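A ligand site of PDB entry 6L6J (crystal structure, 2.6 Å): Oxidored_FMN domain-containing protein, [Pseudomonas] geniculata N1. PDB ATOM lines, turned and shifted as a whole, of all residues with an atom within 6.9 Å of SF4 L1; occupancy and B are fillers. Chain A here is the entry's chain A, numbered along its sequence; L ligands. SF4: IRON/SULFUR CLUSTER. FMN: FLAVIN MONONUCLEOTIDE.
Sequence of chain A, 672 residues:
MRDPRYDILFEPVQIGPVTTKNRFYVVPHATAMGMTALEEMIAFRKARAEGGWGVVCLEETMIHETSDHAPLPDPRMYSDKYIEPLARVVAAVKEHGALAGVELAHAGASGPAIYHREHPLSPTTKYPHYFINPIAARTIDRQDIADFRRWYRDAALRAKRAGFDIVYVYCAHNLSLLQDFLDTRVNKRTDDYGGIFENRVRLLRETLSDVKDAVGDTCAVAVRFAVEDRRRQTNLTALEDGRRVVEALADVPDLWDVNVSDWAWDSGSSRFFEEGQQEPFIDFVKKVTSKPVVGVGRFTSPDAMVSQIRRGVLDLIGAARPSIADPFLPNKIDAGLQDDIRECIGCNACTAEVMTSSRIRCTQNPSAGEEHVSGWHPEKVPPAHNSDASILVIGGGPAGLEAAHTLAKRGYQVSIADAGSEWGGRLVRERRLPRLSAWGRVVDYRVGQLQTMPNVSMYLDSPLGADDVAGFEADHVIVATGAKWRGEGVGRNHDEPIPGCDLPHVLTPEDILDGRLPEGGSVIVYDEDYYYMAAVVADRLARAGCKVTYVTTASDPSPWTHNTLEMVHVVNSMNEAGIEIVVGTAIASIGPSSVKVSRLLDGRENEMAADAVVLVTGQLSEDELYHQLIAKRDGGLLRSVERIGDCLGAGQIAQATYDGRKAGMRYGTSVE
The backbone carbonyl oxygen of Ile 324 lies within hydrogen-bond range of the side-chain amide nitrogen of Asn 365 (2.8 Å).
The backbone NH (N) of Gln 364 sits close to the side-chain sulfur (SG) of Cys 362 (3.3 Å).
SG of Cys 347 lies close to N of Ala 349 (3.6 Å).
NH1 of Arg 321 is in hydrogen-bond range of OD1 of Asn 348.
SG of Cys 344 sits close to N of Gly 346 (3.3 Å).
The side-chain hydroxyl of Thr 363 sits close to the side-chain sulfur of Cys 347, 3.0 Å away.
The backbone NH (N) of Asn 365 lies close to the side-chain sulfur (SG) of Cys 362 (3.4 Å).
NE of Arg 321 is in salt-bridge range of O3P of FMN L2 (2.7 Å).
The backbone NH of Thr 363 sits close to a sulfur (S2) of SF4 L1.
The backbone NH (N) of Cys 347 sits close to a sulfur (S3) of SF4 L1 (3.7 Å).
The backbone NH (N) of Arg 321 sits at hydrogen-bond distance from an oxygen (O3P) of FMN L2 (3.2 Å).
An iron atom (FE3) of SF4 L1 is bound by the side-chain sulfur (SG) of Cys 362 (2.0 Å).
A sulfur (S4) of SF4 L1 sits close to the backbone NH (N) of Ile 345, 3.7 Å away.
N of Cys 350 sits close to S2 of SF4 L1, at 3.7 Å.
The side-chain sulfur (SG) of Cys 350 is bound to an iron atom (FE4) of SF4 L1 (2.1 Å).
The backbone NH (N) of Ala 320 sits at hydrogen-bond distance from an oxygen (O2P) of FMN L2 (2.9 Å).
FE2 of SF4 L1 is bound by SG of Cys 344 (2.2 Å).
The side-chain sulfur (SG) of Cys 347 is bound to an iron atom (FE1) of SF4 L1.
The backbone NH of Arg 298 lies within hydrogen-bond range of an oxygen (O1P) of FMN L2 (2.9 Å).
N of Asn 348 lies close to S3 of SF4 L1 (3.5 Å).
S1 of SF4 L1 sits close to O of Arg 321 (3.7 Å).
Merely in contact with SF4 L1: Ile 324 (3.6 Å) and Gly 346 (3.9 Å).
Hydrophobic or aromatic side chains within 4 Å of SF4 L1: Ile 324.
Within 4 Å of SF4 L1: Arg 321, Ile 324, Cys 344, Ile 345, Gly 346, Cys 347, Asn 348, Cys 350, Cys 362 and Thr 363.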
ATOM      1  N   ARG A 298      -5.377  33.978  16.487  1.00  0.00           N
ATOM      2  CA  ARG A 298      -5.634  33.762  15.042  1.00  0.00           C
ATOM      3  C   ARG A 298      -4.340  34.017  14.263  1.00  0.00           C
ATOM      4  O   ARG A 298      -4.399  34.697  13.215  1.00  0.00           O
ATOM      5  CB  ARG A 298      -6.788  34.637  14.565  1.00  0.00           C
ATOM      6  CG  ARG A 298      -7.637  33.991  13.481  1.00  0.00           C
ATOM      7  CD  ARG A 298      -8.135  34.958  12.425  1.00  0.00           C
ATOM      8  NE  ARG A 298      -8.819  36.102  13.021  1.00  0.00           N
ATOM      9  CZ  ARG A 298      -8.758  37.348  12.567  1.00  0.00           C
ATOM     10  NH1 ARG A 298      -8.097  37.634  11.461  1.00  0.00           N
ATOM     11  NH2 ARG A 298      -9.372  38.309  13.232  1.00  0.00           N
ATOM     12  N   ALA A 320      -5.680  27.264  16.531  1.00  0.00           N
ATOM     13  CA  ALA A 320      -6.786  26.361  16.114  1.00  0.00           C
ATOM     14  C   ALA A 320      -7.147  26.720  14.663  1.00  0.00           C
ATOM     15  O   ALA A 320      -6.763  25.968  13.772  1.00  0.00           O
ATOM     16  CB  ALA A 320      -7.971  26.461  17.062  1.00  0.00           C
ATOM     17  N   ARG A 321      -7.807  27.854  14.465  1.00  0.00           N
ATOM     18  CA  ARG A 321      -8.394  28.232  13.143  1.00  0.00           C
ATOM     19  C   ARG A 321      -7.308  28.240  12.076  1.00  0.00           C
ATOM     20  O   ARG A 321      -7.476  27.669  11.008  1.00  0.00           O
ATOM     21  CB  ARG A 321      -9.174  29.551  13.214  1.00  0.00           C
ATOM     22  CG  ARG A 321     -10.610  29.361  13.679  1.00  0.00           C
ATOM     23  CD  ARG A 321     -11.338  30.615  14.051  1.00  0.00           C
ATOM     24  NE  ARG A 321     -10.572  31.425  15.004  1.00  0.00           N
ATOM     25  CZ  ARG A 321     -10.878  32.670  15.316  1.00  0.00           C
ATOM     26  NH1 ARG A 321     -11.948  33.252  14.798  1.00  0.00           N
ATOM     27  NH2 ARG A 321     -10.110  33.348  16.127  1.00  0.00           N
ATOM     28  N   PRO A 322      -6.147  28.887  12.308  1.00  0.00           N
ATOM     29  CA  PRO A 322      -5.078  28.884  11.312  1.00  0.00           C
ATOM     30  C   PRO A 322      -4.653  27.474  10.876  1.00  0.00           C
ATOM     31  O   PRO A 322      -4.451  27.258   9.664  1.00  0.00           O
ATOM     32  CB  PRO A 322      -3.934  29.641  12.008  1.00  0.00           C
ATOM     33  CG  PRO A 322      -4.680  30.548  12.968  1.00  0.00           C
ATOM     34  CD  PRO A 322      -5.833  29.720  13.478  1.00  0.00           C
ATOM     35  N   SER A 323      -4.592  26.529  11.823  1.00  0.00           N
ATOM     36  CA  SER A 323      -4.276  25.111  11.556  1.00  0.00           C
ATOM     37  C   SER A 323      -5.404  24.412  10.776  1.00  0.00           C
ATOM     38  O   SER A 323      -5.150  23.338  10.210  1.00  0.00           O
ATOM     39  CB  SER A 323      -3.941  24.370  12.839  1.00  0.00           C
ATOM     40  OG  SER A 323      -5.072  24.256  13.680  1.00  0.00           O
ATOM     41  N   ILE A 324      -6.633  24.919  10.836  1.00  0.00           N
ATOM     42  CA  ILE A 324      -7.821  24.356  10.142  1.00  0.00           C
ATOM     43  C   ILE A 324      -7.709  24.757   8.675  1.00  0.00           C
ATOM     44  O   ILE A 324      -7.810  23.877   7.797  1.00  0.00           O
ATOM     45  CB  ILE A 324      -9.136  24.844  10.793  1.00  0.00           C
ATOM     46  CG1 ILE A 324      -9.395  24.120  12.120  1.00  0.00           C
ATOM     47  CG2 ILE A 324     -10.326  24.705   9.839  1.00  0.00           C
ATOM     48  CD1 ILE A 324     -10.529  24.735  12.960  1.00  0.00           C
ATOM     49  N   ALA A 325      -7.468  26.042   8.448  1.00  0.00           N
ATOM     50  CA  ALA A 325      -7.324  26.728   7.133  1.00  0.00           C
ATOM     51  C   ALA A 325      -6.058  26.270   6.430  1.00  0.00           C
ATOM     52  O   ALA A 325      -6.105  26.144   5.207  1.00  0.00           O
ATOM     53  CB  ALA A 325      -7.301  28.230   7.340  1.00  0.00           C
ATOM     54  N   GLU A 343      -4.545  31.719   4.408  1.00  0.00           N
ATOM     55  CA  GLU A 343      -4.811  32.539   5.635  1.00  0.00           C
ATOM     56  C   GLU A 343      -6.274  32.425   6.043  1.00  0.00           C
ATOM     57  O   GLU A 343      -7.141  32.662   5.195  1.00  0.00           O
ATOM     58  CB  GLU A 343      -4.504  34.003   5.361  1.00  0.00           C
ATOM     59  CG  GLU A 343      -3.082  34.241   4.965  1.00  0.00           C
ATOM     60  CD  GLU A 343      -2.835  35.711   4.746  1.00  0.00           C
ATOM     61  OE1 GLU A 343      -3.427  36.519   5.497  1.00  0.00           O
ATOM     62  OE2 GLU A 343      -2.100  36.027   3.801  1.00  0.00           O
ATOM     63  N   CYS A 344      -6.531  32.090   7.307  1.00  0.00           N
ATOM     64  CA  CYS A 344      -7.880  32.099   7.927  1.00  0.00           C
ATOM     65  C   CYS A 344      -8.485  33.498   7.746  1.00  0.00           C
ATOM     66  O   CYS A 344      -7.733  34.484   7.783  1.00  0.00           O
ATOM     67  CB  CYS A 344      -7.816  31.707   9.404  1.00  0.00           C
ATOM     68  SG  CYS A 344      -9.359  31.978  10.342  1.00  0.00           S
ATOM     69  N   ILE A 345      -9.792  33.595   7.525  1.00  0.00           N
ATOM     70  CA  ILE A 345     -10.493  34.875   7.281  1.00  0.00           C
ATOM     71  C   ILE A 345     -11.403  35.199   8.467  1.00  0.00           C
ATOM     72  O   ILE A 345     -12.020  36.248   8.416  1.00  0.00           O
ATOM     73  CB  ILE A 345     -11.271  34.838   5.950  1.00  0.00           C
ATOM     74  CG1 ILE A 345     -12.532  33.965   6.035  1.00  0.00           C
ATOM     75  CG2 ILE A 345     -10.320  34.410   4.826  1.00  0.00           C
ATOM     76  CD1 ILE A 345     -13.355  33.928   4.758  1.00  0.00           C
ATOM     77  N   GLY A 346     -11.485  34.312   9.443  1.00  0.00           N
ATOM     78  CA  GLY A 346     -12.244  34.541  10.696  1.00  0.00           C
ATOM     79  C   GLY A 346     -13.739  34.608  10.484  1.00  0.00           C
ATOM     80  O   GLY A 346     -14.373  35.323  11.254  1.00  0.00           O
ATOM     81  N   CYS A 347     -14.286  33.831   9.531  1.00  0.00           N
ATOM     82  CA  CYS A 347     -15.745  33.746   9.192  1.00  0.00           C
ATOM     83  C   CYS A 347     -16.486  32.936  10.255  1.00  0.00           C
ATOM     84  O   CYS A 347     -17.734  33.108  10.346  1.00  0.00           O
ATOM     85  CB  CYS A 347     -16.003  33.114   7.836  1.00  0.00           C
ATOM     86  SG  CYS A 347     -15.277  31.465   7.678  1.00  0.00           S
ATOM     87  N   ASN A 348     -15.743  32.089  10.978  1.00  0.00           N
ATOM     88  CA  ASN A 348     -16.253  31.159  12.037  1.00  0.00           C
ATOM     89  C   ASN A 348     -17.314  30.194  11.466  1.00  0.00           C
ATOM     90  O   ASN A 348     -18.165  29.712  12.241  1.00  0.00           O
ATOM     91  CB  ASN A 348     -16.761  31.926  13.243  1.00  0.00           C
ATOM     92  CG  ASN A 348     -15.658  32.364  14.187  1.00  0.00           C
ATOM     93  OD1 ASN A 348     -14.472  32.163  13.903  1.00  0.00           O
ATOM     94  ND2 ASN A 348     -16.024  32.967  15.317  1.00  0.00           N
ATOM     95  N   ALA A 349     -17.241  29.858  10.173  1.00  0.00           N
ATOM     96  CA  ALA A 349     -18.060  28.772   9.567  1.00  0.00           C
ATOM     97  C   ALA A 349     -17.661  27.416  10.175  1.00  0.00           C
ATOM     98  O   ALA A 349     -18.528  26.521  10.189  1.00  0.00           O
ATOM     99  CB  ALA A 349     -17.904  28.803   8.071  1.00  0.00           C
ATOM    100  N   CYS A 350     -16.409  27.247  10.631  1.00  0.00           N
ATOM    101  CA  CYS A 350     -15.918  26.037  11.377  1.00  0.00           C
ATOM    102  C   CYS A 350     -16.666  25.915  12.707  1.00  0.00           C
ATOM    103  O   CYS A 350     -17.199  24.846  13.047  1.00  0.00           O
ATOM    104  CB  CYS A 350     -14.406  26.110  11.619  1.00  0.00           C
ATOM    105  SG  CYS A 350     -13.788  27.696  12.224  1.00  0.00           S
ATOM    106  N   THR A 351     -16.728  27.026  13.428  1.00  0.00           N
ATOM    107  CA  THR A 351     -17.491  27.240  14.688  1.00  0.00           C
ATOM    108  C   THR A 351     -18.971  26.885  14.452  1.00  0.00           C
ATOM    109  O   THR A 351     -19.600  26.210  15.345  1.00  0.00           O
ATOM    110  CB  THR A 351     -17.183  28.687  15.121  1.00  0.00           C
ATOM    111  OG1 THR A 351     -15.859  28.638  15.682  1.00  0.00           O
ATOM    112  CG2 THR A 351     -18.160  29.277  16.098  1.00  0.00           C
ATOM    113  N   ILE A 360     -17.142  19.436  11.207  1.00  0.00           N
ATOM    114  CA  ILE A 360     -16.455  20.750  10.954  1.00  0.00           C
ATOM    115  C   ILE A 360     -16.226  20.946   9.447  1.00  0.00           C
ATOM    116  O   ILE A 360     -16.050  19.960   8.738  1.00  0.00           O
ATOM    117  CB  ILE A 360     -15.144  20.831  11.759  1.00  0.00           C
ATOM    118  CG1 ILE A 360     -14.468  22.207  11.638  1.00  0.00           C
ATOM    119  CG2 ILE A 360     -14.184  19.717  11.341  1.00  0.00           C
ATOM    120  CD1 ILE A 360     -13.327  22.421  12.606  1.00  0.00           C
ATOM    121  N   ARG A 361     -16.245  22.195   9.000  1.00  0.00           N
ATOM    122  CA  ARG A 361     -15.850  22.612   7.617  1.00  0.00           C
ATOM    123  C   ARG A 361     -15.046  23.910   7.719  1.00  0.00           C
ATOM    124  O   ARG A 361     -15.099  24.539   8.781  1.00  0.00           O
ATOM    125  CB  ARG A 361     -17.070  22.835   6.721  1.00  0.00           C
ATOM    126  CG  ARG A 361     -17.760  24.173   6.931  1.00  0.00           C
ATOM    127  CD  ARG A 361     -19.175  24.179   6.410  1.00  0.00           C
ATOM    128  NE  ARG A 361     -19.202  24.062   4.954  1.00  0.00           N
ATOM    129  CZ  ARG A 361     -20.313  23.919   4.238  1.00  0.00           C
ATOM    130  NH1 ARG A 361     -21.487  23.850   4.845  1.00  0.00           N
ATOM    131  NH2 ARG A 361     -20.242  23.828   2.912  1.00  0.00           N
ATOM    132  N   CYS A 362     -14.399  24.312   6.621  1.00  0.00           N
ATOM    133  CA  CYS A 362     -13.606  25.572   6.525  1.00  0.00           C
ATOM    134  C   CYS A 362     -13.855  26.256   5.176  1.00  0.00           C
ATOM    135  O   CYS A 362     -13.773  25.593   4.127  1.00  0.00           O
ATOM    136  CB  CYS A 362     -12.112  25.309   6.687  1.00  0.00           C
ATOM    137  SG  CYS A 362     -11.089  26.800   6.540  1.00  0.00           S
ATOM    138  N   THR A 363     -14.158  27.544   5.200  1.00  0.00           N
ATOM    139  CA  THR A 363     -14.377  28.366   3.982  1.00  0.00           C
ATOM    140  C   THR A 363     -13.127  28.314   3.077  1.00  0.00           C
ATOM    141  O   THR A 363     -13.291  28.264   1.793  1.00  0.00           O
ATOM    142  CB  THR A 363     -14.725  29.800   4.386  1.00  0.00           C
ATOM    143  OG1 THR A 363     -15.771  29.650   5.347  1.00  0.00           O
ATOM    144  CG2 THR A 363     -15.114  30.644   3.192  1.00  0.00           C
ATOM    145  N   GLN A 364     -11.935  28.367   3.703  1.00  0.00           N
ATOM    146  CA  GLN A 364     -10.654  28.538   2.973  1.00  0.00           C
ATOM    147  C   GLN A 364     -10.169  27.166   2.498  1.00  0.00           C
ATOM    148  O   GLN A 364      -9.728  27.075   1.338  1.00  0.00           O
ATOM    149  CB  GLN A 364      -9.573  29.196   3.840  1.00  0.00           C
ATOM    150  CG  GLN A 364      -9.579  30.716   3.869  1.00  0.00           C
ATOM    151  CD  GLN A 364      -9.124  31.321   2.562  1.00  0.00           C
ATOM    152  OE1 GLN A 364      -9.723  31.083   1.512  1.00  0.00           O
ATOM    153  NE2 GLN A 364      -8.063  32.120   2.621  1.00  0.00           N
ATOM    154  N   ASN A 365     -10.321  26.154   3.338  1.00  0.00           N
ATOM    155  CA  ASN A 365      -9.764  24.793   3.123  1.00  0.00           C
ATOM    156  C   ASN A 365     -10.914  23.794   3.039  1.00  0.00           C
ATOM    157  O   ASN A 365     -11.228  23.139   4.026  1.00  0.00           O
ATOM    158  CB  ASN A 365      -8.737  24.479   4.222  1.00  0.00           C
ATOM    159  CG  ASN A 365      -8.204  23.073   4.184  1.00  0.00           C
ATOM    160  OD1 ASN A 365      -8.191  22.412   3.120  1.00  0.00           O
ATOM    161  ND2 ASN A 365      -7.796  22.586   5.349  1.00  0.00           N
ATOM    162  N   ALA A 368     -10.900  20.405   5.027  1.00  0.00           N
ATOM    163  CA  ALA A 368     -11.153  20.366   6.488  1.00  0.00           C
ATOM    164  C   ALA A 368     -12.464  19.610   6.726  1.00  0.00           C
ATOM    165  O   ALA A 368     -13.481  20.109   6.253  1.00  0.00           O
ATOM    166  CB  ALA A 368     -11.209  21.755   7.078  1.00  0.00           C
ATOM    167  N   VAL A 442      -9.943  34.829   0.647  1.00  0.00           N
ATOM    168  CA  VAL A 442     -10.540  33.754  -0.196  1.00  0.00           C
ATOM    169  C   VAL A 442     -10.157  34.023  -1.671  1.00  0.00           C
ATOM    170  O   VAL A 442      -9.738  33.046  -2.365  1.00  0.00           O
ATOM    171  CB  VAL A 442     -12.065  33.589   0.015  1.00  0.00           C
ATOM    172  CG1 VAL A 442     -12.775  32.893  -1.147  1.00  0.00           C
ATOM    173  CG2 VAL A 442     -12.370  32.846   1.312  1.00  0.00           C
ATOM    174  N   ALA A 654     -18.326  29.415   1.937  1.00  0.00           N
ATOM    175  CA  ALA A 654     -17.788  28.057   2.201  1.00  0.00           C
ATOM    176  C   ALA A 654     -18.353  27.055   1.185  1.00  0.00           C
ATOM    177  O   ALA A 654     -17.604  26.174   0.766  1.00  0.00           O
ATOM    178  CB  ALA A 654     -18.110  27.585   3.591  1.00  0.00           C
HETATM  179 FE1  SF4 L   1     -13.347  30.653   8.314  1.00  0.00          FE
HETATM  180 FE2  SF4 L   1     -10.618  30.329   9.589  1.00  0.00          FE
HETATM  181 FE3  SF4 L   1     -11.728  28.193   7.819  1.00  0.00          FE
HETATM  182 FE4  SF4 L   1     -12.867  28.626  10.589  1.00  0.00          FE
HETATM  183  S1  SF4 L   1     -10.970  28.254   9.825  1.00  0.00           S
HETATM  184  S2  SF4 L   1     -13.673  28.592   8.611  1.00  0.00           S
HETATM  185  S3  SF4 L   1     -12.583  30.703  10.338  1.00  0.00           S
HETATM  186  S4  SF4 L   1     -11.392  30.233   7.600  1.00  0.00           S
HETATM  187  N1  FMN L   2     -11.242  25.275  22.783  1.00  0.00           N
HETATM  188  C2  FMN L   2     -11.287  24.317  23.755  1.00  0.00           C
HETATM  189  O2  FMN L   2     -10.679  24.537  24.801  1.00  0.00           O
HETATM  190  N3  FMN L   2     -11.902  23.132  23.637  1.00  0.00           N
HETATM  191  C4  FMN L   2     -12.554  22.803  22.496  1.00  0.00           C
HETATM  192  O4  FMN L   2     -13.120  21.721  22.391  1.00  0.00           O
HETATM  193  C4A FMN L   2     -12.585  23.804  21.394  1.00  0.00           C
HETATM  194  N5  FMN L   2     -13.226  23.542  20.232  1.00  0.00           N
HETATM  195  C5A FMN L   2     -13.174  24.444  19.220  1.00  0.00           C
HETATM  196  C6  FMN L   2     -13.765  24.151  17.999  1.00  0.00           C
HETATM  197  C7  FMN L   2     -13.677  25.072  16.977  1.00  0.00           C
HETATM  198  C7M FMN L   2     -14.374  24.768  15.701  1.00  0.00           C
HETATM  199  C8  FMN L   2     -12.943  26.331  17.149  1.00  0.00           C
HETATM  200  C8M FMN L   2     -12.876  27.358  16.054  1.00  0.00           C
HETATM  201  C9  FMN L   2     -12.359  26.637  18.342  1.00  0.00           C
HETATM  202  C9A FMN L   2     -12.414  25.739  19.395  1.00  0.00           C
HETATM  203  N10 FMN L   2     -11.777  26.009  20.619  1.00  0.00           N
HETATM  204  C10 FMN L   2     -11.853  25.066  21.606  1.00  0.00           C
HETATM  205  C1' FMN L   2     -11.017  27.280  20.862  1.00  0.00           C
HETATM  206  C2' FMN L   2      -9.624  27.187  20.266  1.00  0.00           C
HETATM  207  O2' FMN L   2      -8.923  26.202  21.001  1.00  0.00           O
HETATM  208  C3' FMN L   2      -8.871  28.475  20.340  1.00  0.00           C
HETATM  209  O3' FMN L   2      -8.634  28.796  21.711  1.00  0.00           O
HETATM  210  C4' FMN L   2      -9.559  29.651  19.653  1.00  0.00           C
HETATM  211  O4' FMN L   2     -10.097  29.235  18.380  1.00  0.00           O
HETATM  212  C5' FMN L   2      -8.617  30.840  19.496  1.00  0.00           C
HETATM  213  O5' FMN L   2      -7.535  30.435  18.671  1.00  0.00           O
HETATM  214  P   FMN L   2      -7.564  30.719  17.074  1.00  0.00           P
HETATM  215  O1P FMN L   2      -7.581  32.221  16.928  1.00  0.00           O
HETATM  216  O2P FMN L   2      -6.300  30.064  16.624  1.00  0.00           O
HETATM  217  O3P FMN L   2      -8.818  30.041  16.570  1.00  0.00           O
